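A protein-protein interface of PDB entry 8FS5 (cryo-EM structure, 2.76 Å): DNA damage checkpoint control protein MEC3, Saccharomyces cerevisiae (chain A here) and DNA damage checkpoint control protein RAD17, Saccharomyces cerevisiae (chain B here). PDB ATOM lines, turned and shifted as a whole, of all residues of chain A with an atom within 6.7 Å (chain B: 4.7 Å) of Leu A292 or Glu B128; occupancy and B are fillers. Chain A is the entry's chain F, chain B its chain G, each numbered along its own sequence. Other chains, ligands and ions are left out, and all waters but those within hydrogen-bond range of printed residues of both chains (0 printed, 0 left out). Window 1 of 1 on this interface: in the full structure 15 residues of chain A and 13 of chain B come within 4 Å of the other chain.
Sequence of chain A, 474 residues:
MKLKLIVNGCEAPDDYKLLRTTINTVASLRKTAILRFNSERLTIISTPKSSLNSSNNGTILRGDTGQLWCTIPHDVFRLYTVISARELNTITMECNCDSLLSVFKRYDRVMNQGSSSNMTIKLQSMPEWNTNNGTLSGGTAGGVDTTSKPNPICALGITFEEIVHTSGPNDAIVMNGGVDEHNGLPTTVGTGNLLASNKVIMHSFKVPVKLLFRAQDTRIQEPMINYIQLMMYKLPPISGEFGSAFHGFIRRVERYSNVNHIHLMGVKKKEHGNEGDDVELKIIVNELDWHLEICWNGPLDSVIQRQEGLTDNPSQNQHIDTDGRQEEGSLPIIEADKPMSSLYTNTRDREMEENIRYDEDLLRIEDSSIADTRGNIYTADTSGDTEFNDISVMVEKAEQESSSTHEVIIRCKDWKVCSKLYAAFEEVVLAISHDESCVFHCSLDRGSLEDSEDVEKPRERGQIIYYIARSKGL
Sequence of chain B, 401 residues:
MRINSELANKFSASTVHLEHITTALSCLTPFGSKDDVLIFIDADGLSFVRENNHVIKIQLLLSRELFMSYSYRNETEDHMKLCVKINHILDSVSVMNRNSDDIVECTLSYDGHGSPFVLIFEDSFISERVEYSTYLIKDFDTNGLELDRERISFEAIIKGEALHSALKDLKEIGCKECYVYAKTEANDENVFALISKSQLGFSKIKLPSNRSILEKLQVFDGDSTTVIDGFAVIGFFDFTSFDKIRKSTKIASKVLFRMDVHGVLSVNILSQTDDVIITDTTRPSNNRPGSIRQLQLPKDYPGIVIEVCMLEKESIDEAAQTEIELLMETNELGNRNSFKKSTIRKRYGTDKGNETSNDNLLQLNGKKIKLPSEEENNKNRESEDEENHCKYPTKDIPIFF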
ATOM      1  N   ARG A 252       9.801  18.778 -27.032  1.00  0.00           N
ATOM      2  CA  ARG A 252      10.811  19.772 -26.688  1.00  0.00           C
ATOM      3  C   ARG A 252      11.816  19.991 -27.816  1.00  0.00           C
ATOM      4  O   ARG A 252      12.403  21.074 -27.919  1.00  0.00           O
ATOM      5  CB  ARG A 252      11.523  19.342 -25.404  1.00  0.00           C
ATOM      6  CG  ARG A 252      12.575  20.307 -24.900  1.00  0.00           C
ATOM      7  CD  ARG A 252      11.997  21.473 -24.093  1.00  0.00           C
ATOM      8  NE  ARG A 252      11.011  21.070 -23.096  1.00  0.00           N
ATOM      9  CZ  ARG A 252       9.697  21.141 -23.261  1.00  0.00           C
ATOM     10  NH1 ARG A 252       9.164  21.604 -24.379  1.00  0.00           N
ATOM     11  NH2 ARG A 252       8.897  20.744 -22.275  1.00  0.00           N
ATOM     12  N   VAL A 253      12.009  18.999 -28.682  1.00  0.00           N
ATOM     13  CA  VAL A 253      12.996  19.098 -29.753  1.00  0.00           C
ATOM     14  C   VAL A 253      12.459  19.951 -30.898  1.00  0.00           C
ATOM     15  O   VAL A 253      13.157  20.184 -31.890  1.00  0.00           O
ATOM     16  CB  VAL A 253      13.402  17.702 -30.258  1.00  0.00           C
ATOM     17  CG1 VAL A 253      13.725  16.788 -29.085  1.00  0.00           C
ATOM     18  CG2 VAL A 253      12.296  17.106 -31.114  1.00  0.00           C
ATOM     19  N   ARG A 255      11.378  23.174 -30.616  1.00  0.00           N
ATOM     20  CA  ARG A 255      11.615  24.601 -30.446  1.00  0.00           C
ATOM     21  C   ARG A 255      12.891  25.066 -31.133  1.00  0.00           C
ATOM     22  O   ARG A 255      13.221  26.254 -31.062  1.00  0.00           O
ATOM     23  CB  ARG A 255      11.660  24.960 -28.957  1.00  0.00           C
ATOM     24  CG  ARG A 255      12.749  24.260 -28.169  1.00  0.00           C
ATOM     25  CD  ARG A 255      12.763  24.723 -26.722  1.00  0.00           C
ATOM     26  NE  ARG A 255      11.453  24.566 -26.100  1.00  0.00           N
ATOM     27  CZ  ARG A 255      11.182  24.863 -24.836  1.00  0.00           C
ATOM     28  NH1 ARG A 255      12.110  25.339 -24.023  1.00  0.00           N
ATOM     29  NH2 ARG A 255       9.947  24.675 -24.378  1.00  0.00           N
ATOM     30  N   TYR A 256      13.612  24.160 -31.787  1.00  0.00           N
ATOM     31  CA  TYR A 256      14.822  24.479 -32.540  1.00  0.00           C
ATOM     32  C   TYR A 256      14.521  24.209 -34.010  1.00  0.00           C
ATOM     33  O   TYR A 256      14.389  23.052 -34.422  1.00  0.00           O
ATOM     34  CB  TYR A 256      15.999  23.650 -32.042  1.00  0.00           C
ATOM     35  CG  TYR A 256      16.045  23.519 -30.539  1.00  0.00           C
ATOM     36  CD1 TYR A 256      16.222  24.632 -29.729  1.00  0.00           C
ATOM     37  CD2 TYR A 256      15.904  22.281 -29.928  1.00  0.00           C
ATOM     38  CE1 TYR A 256      16.261  24.514 -28.353  1.00  0.00           C
ATOM     39  CE2 TYR A 256      15.936  22.154 -28.553  1.00  0.00           C
ATOM     40  CZ  TYR A 256      16.120  23.272 -27.771  1.00  0.00           C
ATOM     41  OH  TYR A 256      16.154  23.148 -26.400  1.00  0.00           O
ATOM     42  N   ILE A 283      17.625  12.021 -25.681  1.00  0.00           N
ATOM     43  CA  ILE A 283      17.609  12.593 -27.023  1.00  0.00           C
ATOM     44  C   ILE A 283      18.820  13.505 -27.151  1.00  0.00           C
ATOM     45  O   ILE A 283      18.997  14.430 -26.349  1.00  0.00           O
ATOM     46  CB  ILE A 283      16.306  13.358 -27.300  1.00  0.00           C
ATOM     47  CG1 ILE A 283      15.126  12.387 -27.388  1.00  0.00           C
ATOM     48  CG2 ILE A 283      16.426  14.172 -28.577  1.00  0.00           C
ATOM     49  CD1 ILE A 283      13.788  13.068 -27.570  1.00  0.00           C
ATOM     50  N   ILE A 284      19.653  13.249 -28.156  1.00  0.00           N
ATOM     51  CA  ILE A 284      20.895  13.986 -28.364  1.00  0.00           C
ATOM     52  C   ILE A 284      20.790  14.715 -29.697  1.00  0.00           C
ATOM     53  O   ILE A 284      20.462  14.111 -30.724  1.00  0.00           O
ATOM     54  CB  ILE A 284      22.120  13.063 -28.333  1.00  0.00           C
ATOM     55  CG1 ILE A 284      22.069  12.145 -27.110  1.00  0.00           C
ATOM     56  CG2 ILE A 284      23.402  13.881 -28.335  1.00  0.00           C
ATOM     57  CD1 ILE A 284      23.207  11.153 -27.045  1.00  0.00           C
ATOM     58  N   VAL A 285      21.067  16.013 -29.679  1.00  0.00           N
ATOM     59  CA  VAL A 285      21.087  16.831 -30.885  1.00  0.00           C
ATOM     60  C   VAL A 285      22.508  17.328 -31.115  1.00  0.00           C
ATOM     61  O   VAL A 285      23.116  17.947 -30.234  1.00  0.00           O
ATOM     62  CB  VAL A 285      20.096  18.005 -30.770  1.00  0.00           C
ATOM     63  CG1 VAL A 285      20.341  19.020 -31.875  1.00  0.00           C
ATOM     64  CG2 VAL A 285      18.664  17.495 -30.813  1.00  0.00           C
ATOM     65  N   ASN A 286      23.043  17.055 -32.307  1.00  0.00           N
ATOM     66  CA  ASN A 286      24.407  17.434 -32.654  1.00  0.00           C
ATOM     67  C   ASN A 286      24.445  18.246 -33.944  1.00  0.00           C
ATOM     68  O   ASN A 286      25.400  18.147 -34.718  1.00  0.00           O
ATOM     69  CB  ASN A 286      25.302  16.201 -32.771  1.00  0.00           C
ATOM     70  CG  ASN A 286      24.664  15.092 -33.584  1.00  0.00           C
ATOM     71  OD1 ASN A 286      24.105  14.145 -33.032  1.00  0.00           O
ATOM     72  ND2 ASN A 286      24.748  15.203 -34.904  1.00  0.00           N
ATOM     73  N   LEU A 288      23.983  21.719 -33.906  1.00  0.00           N
ATOM     74  CA  LEU A 288      24.069  23.092 -33.433  1.00  0.00           C
ATOM     75  C   LEU A 288      25.512  23.402 -33.056  1.00  0.00           C
ATOM     76  O   LEU A 288      26.368  22.516 -32.996  1.00  0.00           O
ATOM     77  CB  LEU A 288      23.143  23.331 -32.231  1.00  0.00           C
ATOM     78  CG  LEU A 288      21.654  23.029 -32.423  1.00  0.00           C
ATOM     79  CD1 LEU A 288      20.920  23.079 -31.092  1.00  0.00           C
ATOM     80  CD2 LEU A 288      21.032  23.998 -33.416  1.00  0.00           C
ATOM     81  N   TRP A 290      26.377  24.209 -30.185  1.00  0.00           N
ATOM     82  CA  TRP A 290      26.516  23.588 -28.879  1.00  0.00           C
ATOM     83  C   TRP A 290      25.998  22.156 -28.936  1.00  0.00           C
ATOM     84  O   TRP A 290      25.206  21.791 -29.809  1.00  0.00           O
ATOM     85  CB  TRP A 290      25.763  24.391 -27.809  1.00  0.00           C
ATOM     86  CG  TRP A 290      24.392  24.843 -28.235  1.00  0.00           C
ATOM     87  CD1 TRP A 290      23.202  24.257 -27.915  1.00  0.00           C
ATOM     88  CD2 TRP A 290      24.072  25.985 -29.041  1.00  0.00           C
ATOM     89  NE1 TRP A 290      22.162  24.955 -28.479  1.00  0.00           N
ATOM     90  CE2 TRP A 290      22.669  26.021 -29.176  1.00  0.00           C
ATOM     91  CE3 TRP A 290      24.833  26.977 -29.666  1.00  0.00           C
ATOM     92  CZ2 TRP A 290      22.014  27.008 -29.908  1.00  0.00           C
ATOM     93  CZ3 TRP A 290      24.181  27.956 -30.394  1.00  0.00           C
ATOM     94  CH2 TRP A 290      22.785  27.964 -30.508  1.00  0.00           C
ATOM     95  N   HIS A 291      26.450  21.344 -27.985  1.00  0.00           N
ATOM     96  CA  HIS A 291      26.050  19.942 -27.883  1.00  0.00           C
ATOM     97  C   HIS A 291      24.888  19.869 -26.901  1.00  0.00           C
ATOM     98  O   HIS A 291      25.072  20.039 -25.691  1.00  0.00           O
ATOM     99  CB  HIS A 291      27.211  19.059 -27.436  1.00  0.00           C
ATOM    100  CG  HIS A 291      26.886  17.597 -27.419  1.00  0.00           C
ATOM    101  ND1 HIS A 291      27.217  16.749 -28.453  1.00  0.00           N
ATOM    102  CD2 HIS A 291      26.254  16.834 -26.495  1.00  0.00           C
ATOM    103  CE1 HIS A 291      26.808  15.525 -28.166  1.00  0.00           C
ATOM    104  NE2 HIS A 291      26.220  15.550 -26.984  1.00  0.00           N
ATOM    105  N   LEU A 292      23.692  19.627 -27.426  1.00  0.00           N
ATOM    106  CA  LEU A 292      22.495  19.540 -26.605  1.00  0.00           C
ATOM    107  C   LEU A 292      22.072  18.090 -26.405  1.00  0.00           C
ATOM    108  O   LEU A 292      22.018  17.306 -27.357  1.00  0.00           O
ATOM    109  CB  LEU A 292      21.354  20.338 -27.230  1.00  0.00           C
ATOM    110  CG  LEU A 292      20.076  20.311 -26.398  1.00  0.00           C
ATOM    111  CD1 LEU A 292      20.334  20.929 -25.042  1.00  0.00           C
ATOM    112  CD2 LEU A 292      18.976  21.056 -27.120  1.00  0.00           C
ATOM    113  N   GLU A 293      21.772  17.744 -25.151  1.00  0.00           N
ATOM    114  CA  GLU A 293      21.283  16.420 -24.775  1.00  0.00           C
ATOM    115  C   GLU A 293      19.973  16.601 -24.002  1.00  0.00           C
ATOM    116  O   GLU A 293      19.952  17.120 -22.883  1.00  0.00           O
ATOM    117  CB  GLU A 293      22.334  15.659 -23.962  1.00  0.00           C
ATOM    118  CG  GLU A 293      21.786  14.580 -23.039  1.00  0.00           C
ATOM    119  CD  GLU A 293      22.824  14.092 -22.048  1.00  0.00           C
ATOM    120  OE1 GLU A 293      22.445  13.687 -20.928  1.00  0.00           O
ATOM    121  OE2 GLU A 293      24.024  14.113 -22.391  1.00  0.00           O
ATOM    122  N   ILE A 294      18.867  16.196 -24.623  1.00  0.00           N
ATOM    123  CA  ILE A 294      17.556  16.269 -23.986  1.00  0.00           C
ATOM    124  C   ILE A 294      17.284  14.956 -23.264  1.00  0.00           C
ATOM    125  O   ILE A 294      17.040  13.924 -23.899  1.00  0.00           O
ATOM    126  CB  ILE A 294      16.443  16.587 -25.004  1.00  0.00           C
ATOM    127  CG1 ILE A 294      16.803  17.812 -25.852  1.00  0.00           C
ATOM    128  CG2 ILE A 294      15.123  16.813 -24.291  1.00  0.00           C
ATOM    129  CD1 ILE A 294      17.394  17.486 -27.214  1.00  0.00           C
ATOM    130  N   CYS A 295      17.316  14.988 -21.935  1.00  0.00           N
ATOM    131  CA  CYS A 295      17.203  13.780 -21.135  1.00  0.00           C
ATOM    132  C   CYS A 295      15.837  13.691 -20.456  1.00  0.00           C
ATOM    133  O   CYS A 295      15.047  14.637 -20.449  1.00  0.00           O
ATOM    134  CB  CYS A 295      18.317  13.730 -20.089  1.00  0.00           C
ATOM    135  SG  CYS A 295      18.277  12.268 -19.032  1.00  0.00           S
ATOM    136  N   ASN A 297      14.509  12.216 -16.736  1.00  0.00           N
ATOM    137  CA  ASN A 297      14.796  11.649 -15.426  1.00  0.00           C
ATOM    138  C   ASN A 297      13.577  11.018 -14.769  1.00  0.00           C
ATOM    139  O   ASN A 297      13.688  10.511 -13.649  1.00  0.00           O
ATOM    140  CB  ASN A 297      15.371  12.722 -14.498  1.00  0.00           C
ATOM    141  CG  ASN A 297      16.147  13.779 -15.245  1.00  0.00           C
ATOM    142  OD1 ASN A 297      17.251  13.528 -15.727  1.00  0.00           O
ATOM    143  ND2 ASN A 297      15.573  14.972 -15.349  1.00  0.00           N
ATOM    144  N   MET B  96      15.965  27.861 -23.746  1.00  0.00           N
ATOM    145  CA  MET B  96      15.798  27.195 -22.456  1.00  0.00           C
ATOM    146  C   MET B  96      14.826  27.966 -21.570  1.00  0.00           C
ATOM    147  O   MET B  96      14.000  27.370 -20.870  1.00  0.00           O
ATOM    148  CB  MET B  96      17.145  27.043 -21.747  1.00  0.00           C
ATOM    149  CG  MET B  96      18.317  26.743 -22.652  1.00  0.00           C
ATOM    150  SD  MET B  96      19.629  25.771 -21.893  1.00  0.00           S
ATOM    151  CE  MET B  96      18.801  24.207 -21.708  1.00  0.00           C
ATOM    152  N   LEU B 119      26.063  22.991 -18.781  1.00  0.00           N
ATOM    153  CA  LEU B 119      25.003  23.817 -18.202  1.00  0.00           C
ATOM    154  C   LEU B 119      23.718  22.991 -18.203  1.00  0.00           C
ATOM    155  O   LEU B 119      22.982  22.978 -19.194  1.00  0.00           O
ATOM    156  CB  LEU B 119      24.854  25.119 -18.986  1.00  0.00           C
ATOM    157  CG  LEU B 119      24.009  26.248 -18.398  1.00  0.00           C
ATOM    158  CD1 LEU B 119      24.819  27.529 -18.325  1.00  0.00           C
ATOM    159  CD2 LEU B 119      22.773  26.454 -19.252  1.00  0.00           C
ATOM    160  N   ILE B 120      23.448  22.306 -17.093  1.00  0.00           N
ATOM    161  CA  ILE B 120      22.304  21.404 -17.012  1.00  0.00           C
ATOM    162  C   ILE B 120      21.100  22.142 -16.444  1.00  0.00           C
ATOM    163  O   ILE B 120      21.194  22.825 -15.417  1.00  0.00           O
ATOM    164  CB  ILE B 120      22.642  20.162 -16.166  1.00  0.00           C
ATOM    165  CG1 ILE B 120      23.955  19.525 -16.624  1.00  0.00           C
ATOM    166  CG2 ILE B 120      21.516  19.142 -16.245  1.00  0.00           C
ATOM    167  CD1 ILE B 120      25.116  19.779 -15.691  1.00  0.00           C
ATOM    168  N   PHE B 121      19.959  21.999 -17.116  1.00  0.00           N
ATOM    169  CA  PHE B 121      18.681  22.576 -16.696  1.00  0.00           C
ATOM    170  C   PHE B 121      17.710  21.426 -16.435  1.00  0.00           C
ATOM    171  O   PHE B 121      17.094  20.902 -17.364  1.00  0.00           O
ATOM    172  CB  PHE B 121      18.131  23.533 -17.757  1.00  0.00           C
ATOM    173  CG  PHE B 121      18.606  24.950 -17.611  1.00  0.00           C
ATOM    174  CD1 PHE B 121      19.801  25.236 -16.974  1.00  0.00           C
ATOM    175  CD2 PHE B 121      17.849  25.998 -18.107  1.00  0.00           C
ATOM    176  CE1 PHE B 121      20.233  26.540 -16.839  1.00  0.00           C
ATOM    177  CE2 PHE B 121      18.279  27.304 -17.977  1.00  0.00           C
ATOM    178  CZ  PHE B 121      19.474  27.574 -17.344  1.00  0.00           C
ATOM    179  N   ILE B 126      12.575  16.818 -17.138  1.00  0.00           N
ATOM    180  CA  ILE B 126      13.495  16.963 -18.259  1.00  0.00           C
ATOM    181  C   ILE B 126      14.813  17.513 -17.739  1.00  0.00           C
ATOM    182  O   ILE B 126      14.830  18.473 -16.958  1.00  0.00           O
ATOM    183  CB  ILE B 126      12.908  17.891 -19.339  1.00  0.00           C
ATOM    184  CG1 ILE B 126      11.414  17.619 -19.528  1.00  0.00           C
ATOM    185  CG2 ILE B 126      13.658  17.723 -20.651  1.00  0.00           C
ATOM    186  CD1 ILE B 126      10.792  18.413 -20.649  1.00  0.00           C
ATOM    187  N   SER B 127      15.920  16.914 -18.173  1.00  0.00           N
ATOM    188  CA  SER B 127      17.259  17.372 -17.799  1.00  0.00           C
ATOM    189  C   SER B 127      17.991  17.777 -19.073  1.00  0.00           C
ATOM    190  O   SER B 127      18.714  16.972 -19.665  1.00  0.00           O
ATOM    191  CB  SER B 127      18.033  16.296 -17.046  1.00  0.00           C
ATOM    192  OG  SER B 127      19.430  16.479 -17.192  1.00  0.00           O
ATOM    193  N   GLU B 128      17.801  19.026 -19.487  1.00  0.00           N
ATOM    194  CA  GLU B 128      18.521  19.553 -20.635  1.00  0.00           C
ATOM    195  C   GLU B 128      19.993  19.719 -20.284  1.00  0.00           C
ATOM    196  O   GLU B 128      20.330  20.265 -19.230  1.00  0.00           O
ATOM    197  CB  GLU B 128      17.927  20.892 -21.053  1.00  0.00           C
ATOM    198  CG  GLU B 128      16.500  20.825 -21.554  1.00  0.00           C
ATOM    199  CD  GLU B 128      16.404  21.074 -23.040  1.00  0.00           C
ATOM    200  OE1 GLU B 128      15.277  21.136 -23.561  1.00  0.00           O
ATOM    201  OE2 GLU B 128      17.457  21.213 -23.691  1.00  0.00           O
ATOM    202  N   ARG B 129      20.873  19.250 -21.165  1.00  0.00           N
ATOM    203  CA  ARG B 129      22.312  19.335 -20.952  1.00  0.00           C
ATOM    204  C   ARG B 129      22.950  19.992 -22.166  1.00  0.00           C
ATOM    205  O   ARG B 129      22.844  19.473 -23.282  1.00  0.00           O
ATOM    206  CB  ARG B 129      22.913  17.951 -20.699  1.00  0.00           C
ATOM    207  CG  ARG B 129      24.427  17.943 -20.562  1.00  0.00           C
ATOM    208  CD  ARG B 129      24.955  16.527 -20.433  1.00  0.00           C
ATOM    209  NE  ARG B 129      26.411  16.480 -20.464  1.00  0.00           N
ATOM    210  CZ  ARG B 129      27.180  16.433 -19.385  1.00  0.00           C
ATOM    211  NH1 ARG B 129      26.661  16.429 -18.168  1.00  0.00           N
ATOM    212  NH2 ARG B 129      28.501  16.394 -19.529  1.00  0.00           N
ATOM    213  N   VAL B 130      23.605  21.129 -21.947  1.00  0.00           N
ATOM    214  CA  VAL B 130      24.269  21.886 -23.002  1.00  0.00           C
ATOM    215  C   VAL B 130      25.755  21.935 -22.679  1.00  0.00           C
ATOM    216  O   VAL B 130      26.144  22.355 -21.582  1.00  0.00           O
ATOM    217  CB  VAL B 130      23.691  23.303 -23.139  1.00  0.00           C
ATOM    218  CG1 VAL B 130      23.984  23.864 -24.519  1.00  0.00           C
ATOM    219  CG2 VAL B 130      22.196  23.300 -22.868  1.00  0.00           C
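The backbone NH (N) of Val A285 sits at hydrogen-bond distance from the backbone carbonyl oxygen (O) of Leu A292, 2.8 Å away.
SG of Cys A295 lies within hydrogen-bond range of OD1 of Asn A297, at 3.7 Å.
The backbone carbonyl oxygen (O) of Val B130 lies within hydrogen-bond range of the backbone NH (N) of Leu B119 (2.9 Å).
O of Glu B128 sits at hydrogen-bond distance from N of Phe B121, 2.8 Å away.
Val A285 touches none of the printed residues of chain B.
Of the printed residues of chain B, Trp A290 touches Val B130 (3.5 Å).
Of the printed residues of chain B, Glu A293 touches Ser B127 (3.5 Å), Glu B128 (3.6 Å) and Arg B129 (2.8 Å).
Ile A294 touches none of the printed residues of chain B.
Of the printed residues of chain A, Glu B128 touches Arg A252 (3.1 Å), Tyr A256 (3.6 Å), Leu A292 (3.2 Å) and Glu A293 (3.6 Å).
Of the printed residues of chain A, Arg B129 touches His A291, Leu A292 and Glu A293.
The nearest printed residue of chain B that does not touch Leu A292 is Met B96 (4.9 Å).
The nearest residue of chain A that does not touch Glu B128 is Ile A294 (4.1 Å).
Of the 9 printed residues of chain B, 5 touch a printed residue of chain A.
Of the 16 printed residues of chain A, 8 touch a printed residue of chain B.
Among the printed residues, Asp or Glu carboxylates within 4 Å of a Lys or Arg side-chain nitrogen of the other chain: Glu A293 with Arg B129.
Among the printed residues, merely in contact across the chains: Arg A252 with Glu B128, Leu A292 with Glu B128, Leu A292 with Arg B129, His A291 with Val B130, Cys A295 with Ile B126, Arg A252 with Ile B126, Trp A290 with Val B130, Asn A297 with Ile B126, Tyr A256 with Glu B128, Glu A293 with Glu B128 and Leu A292 with Val B130.
NE of Arg B129 lies within salt-bridge range of OE2 of Glu A293 (3.9 Å).
N of Cys A295 lies close to O of Ser B127.
The side-chain amide nitrogen (ND2) of Asn A297 sits close to the backbone NH (N) of Ser B127, 3.4 Å away.
The backbone carbonyl oxygen (O) of His A291 lies close to the backbone carbonyl oxygen (O) of Arg B129, at 3.3 Å.
The backbone carbonyl oxygen of Ser B127 sits close to the backbone carbonyl oxygen of Glu A293, 3.5 Å away.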
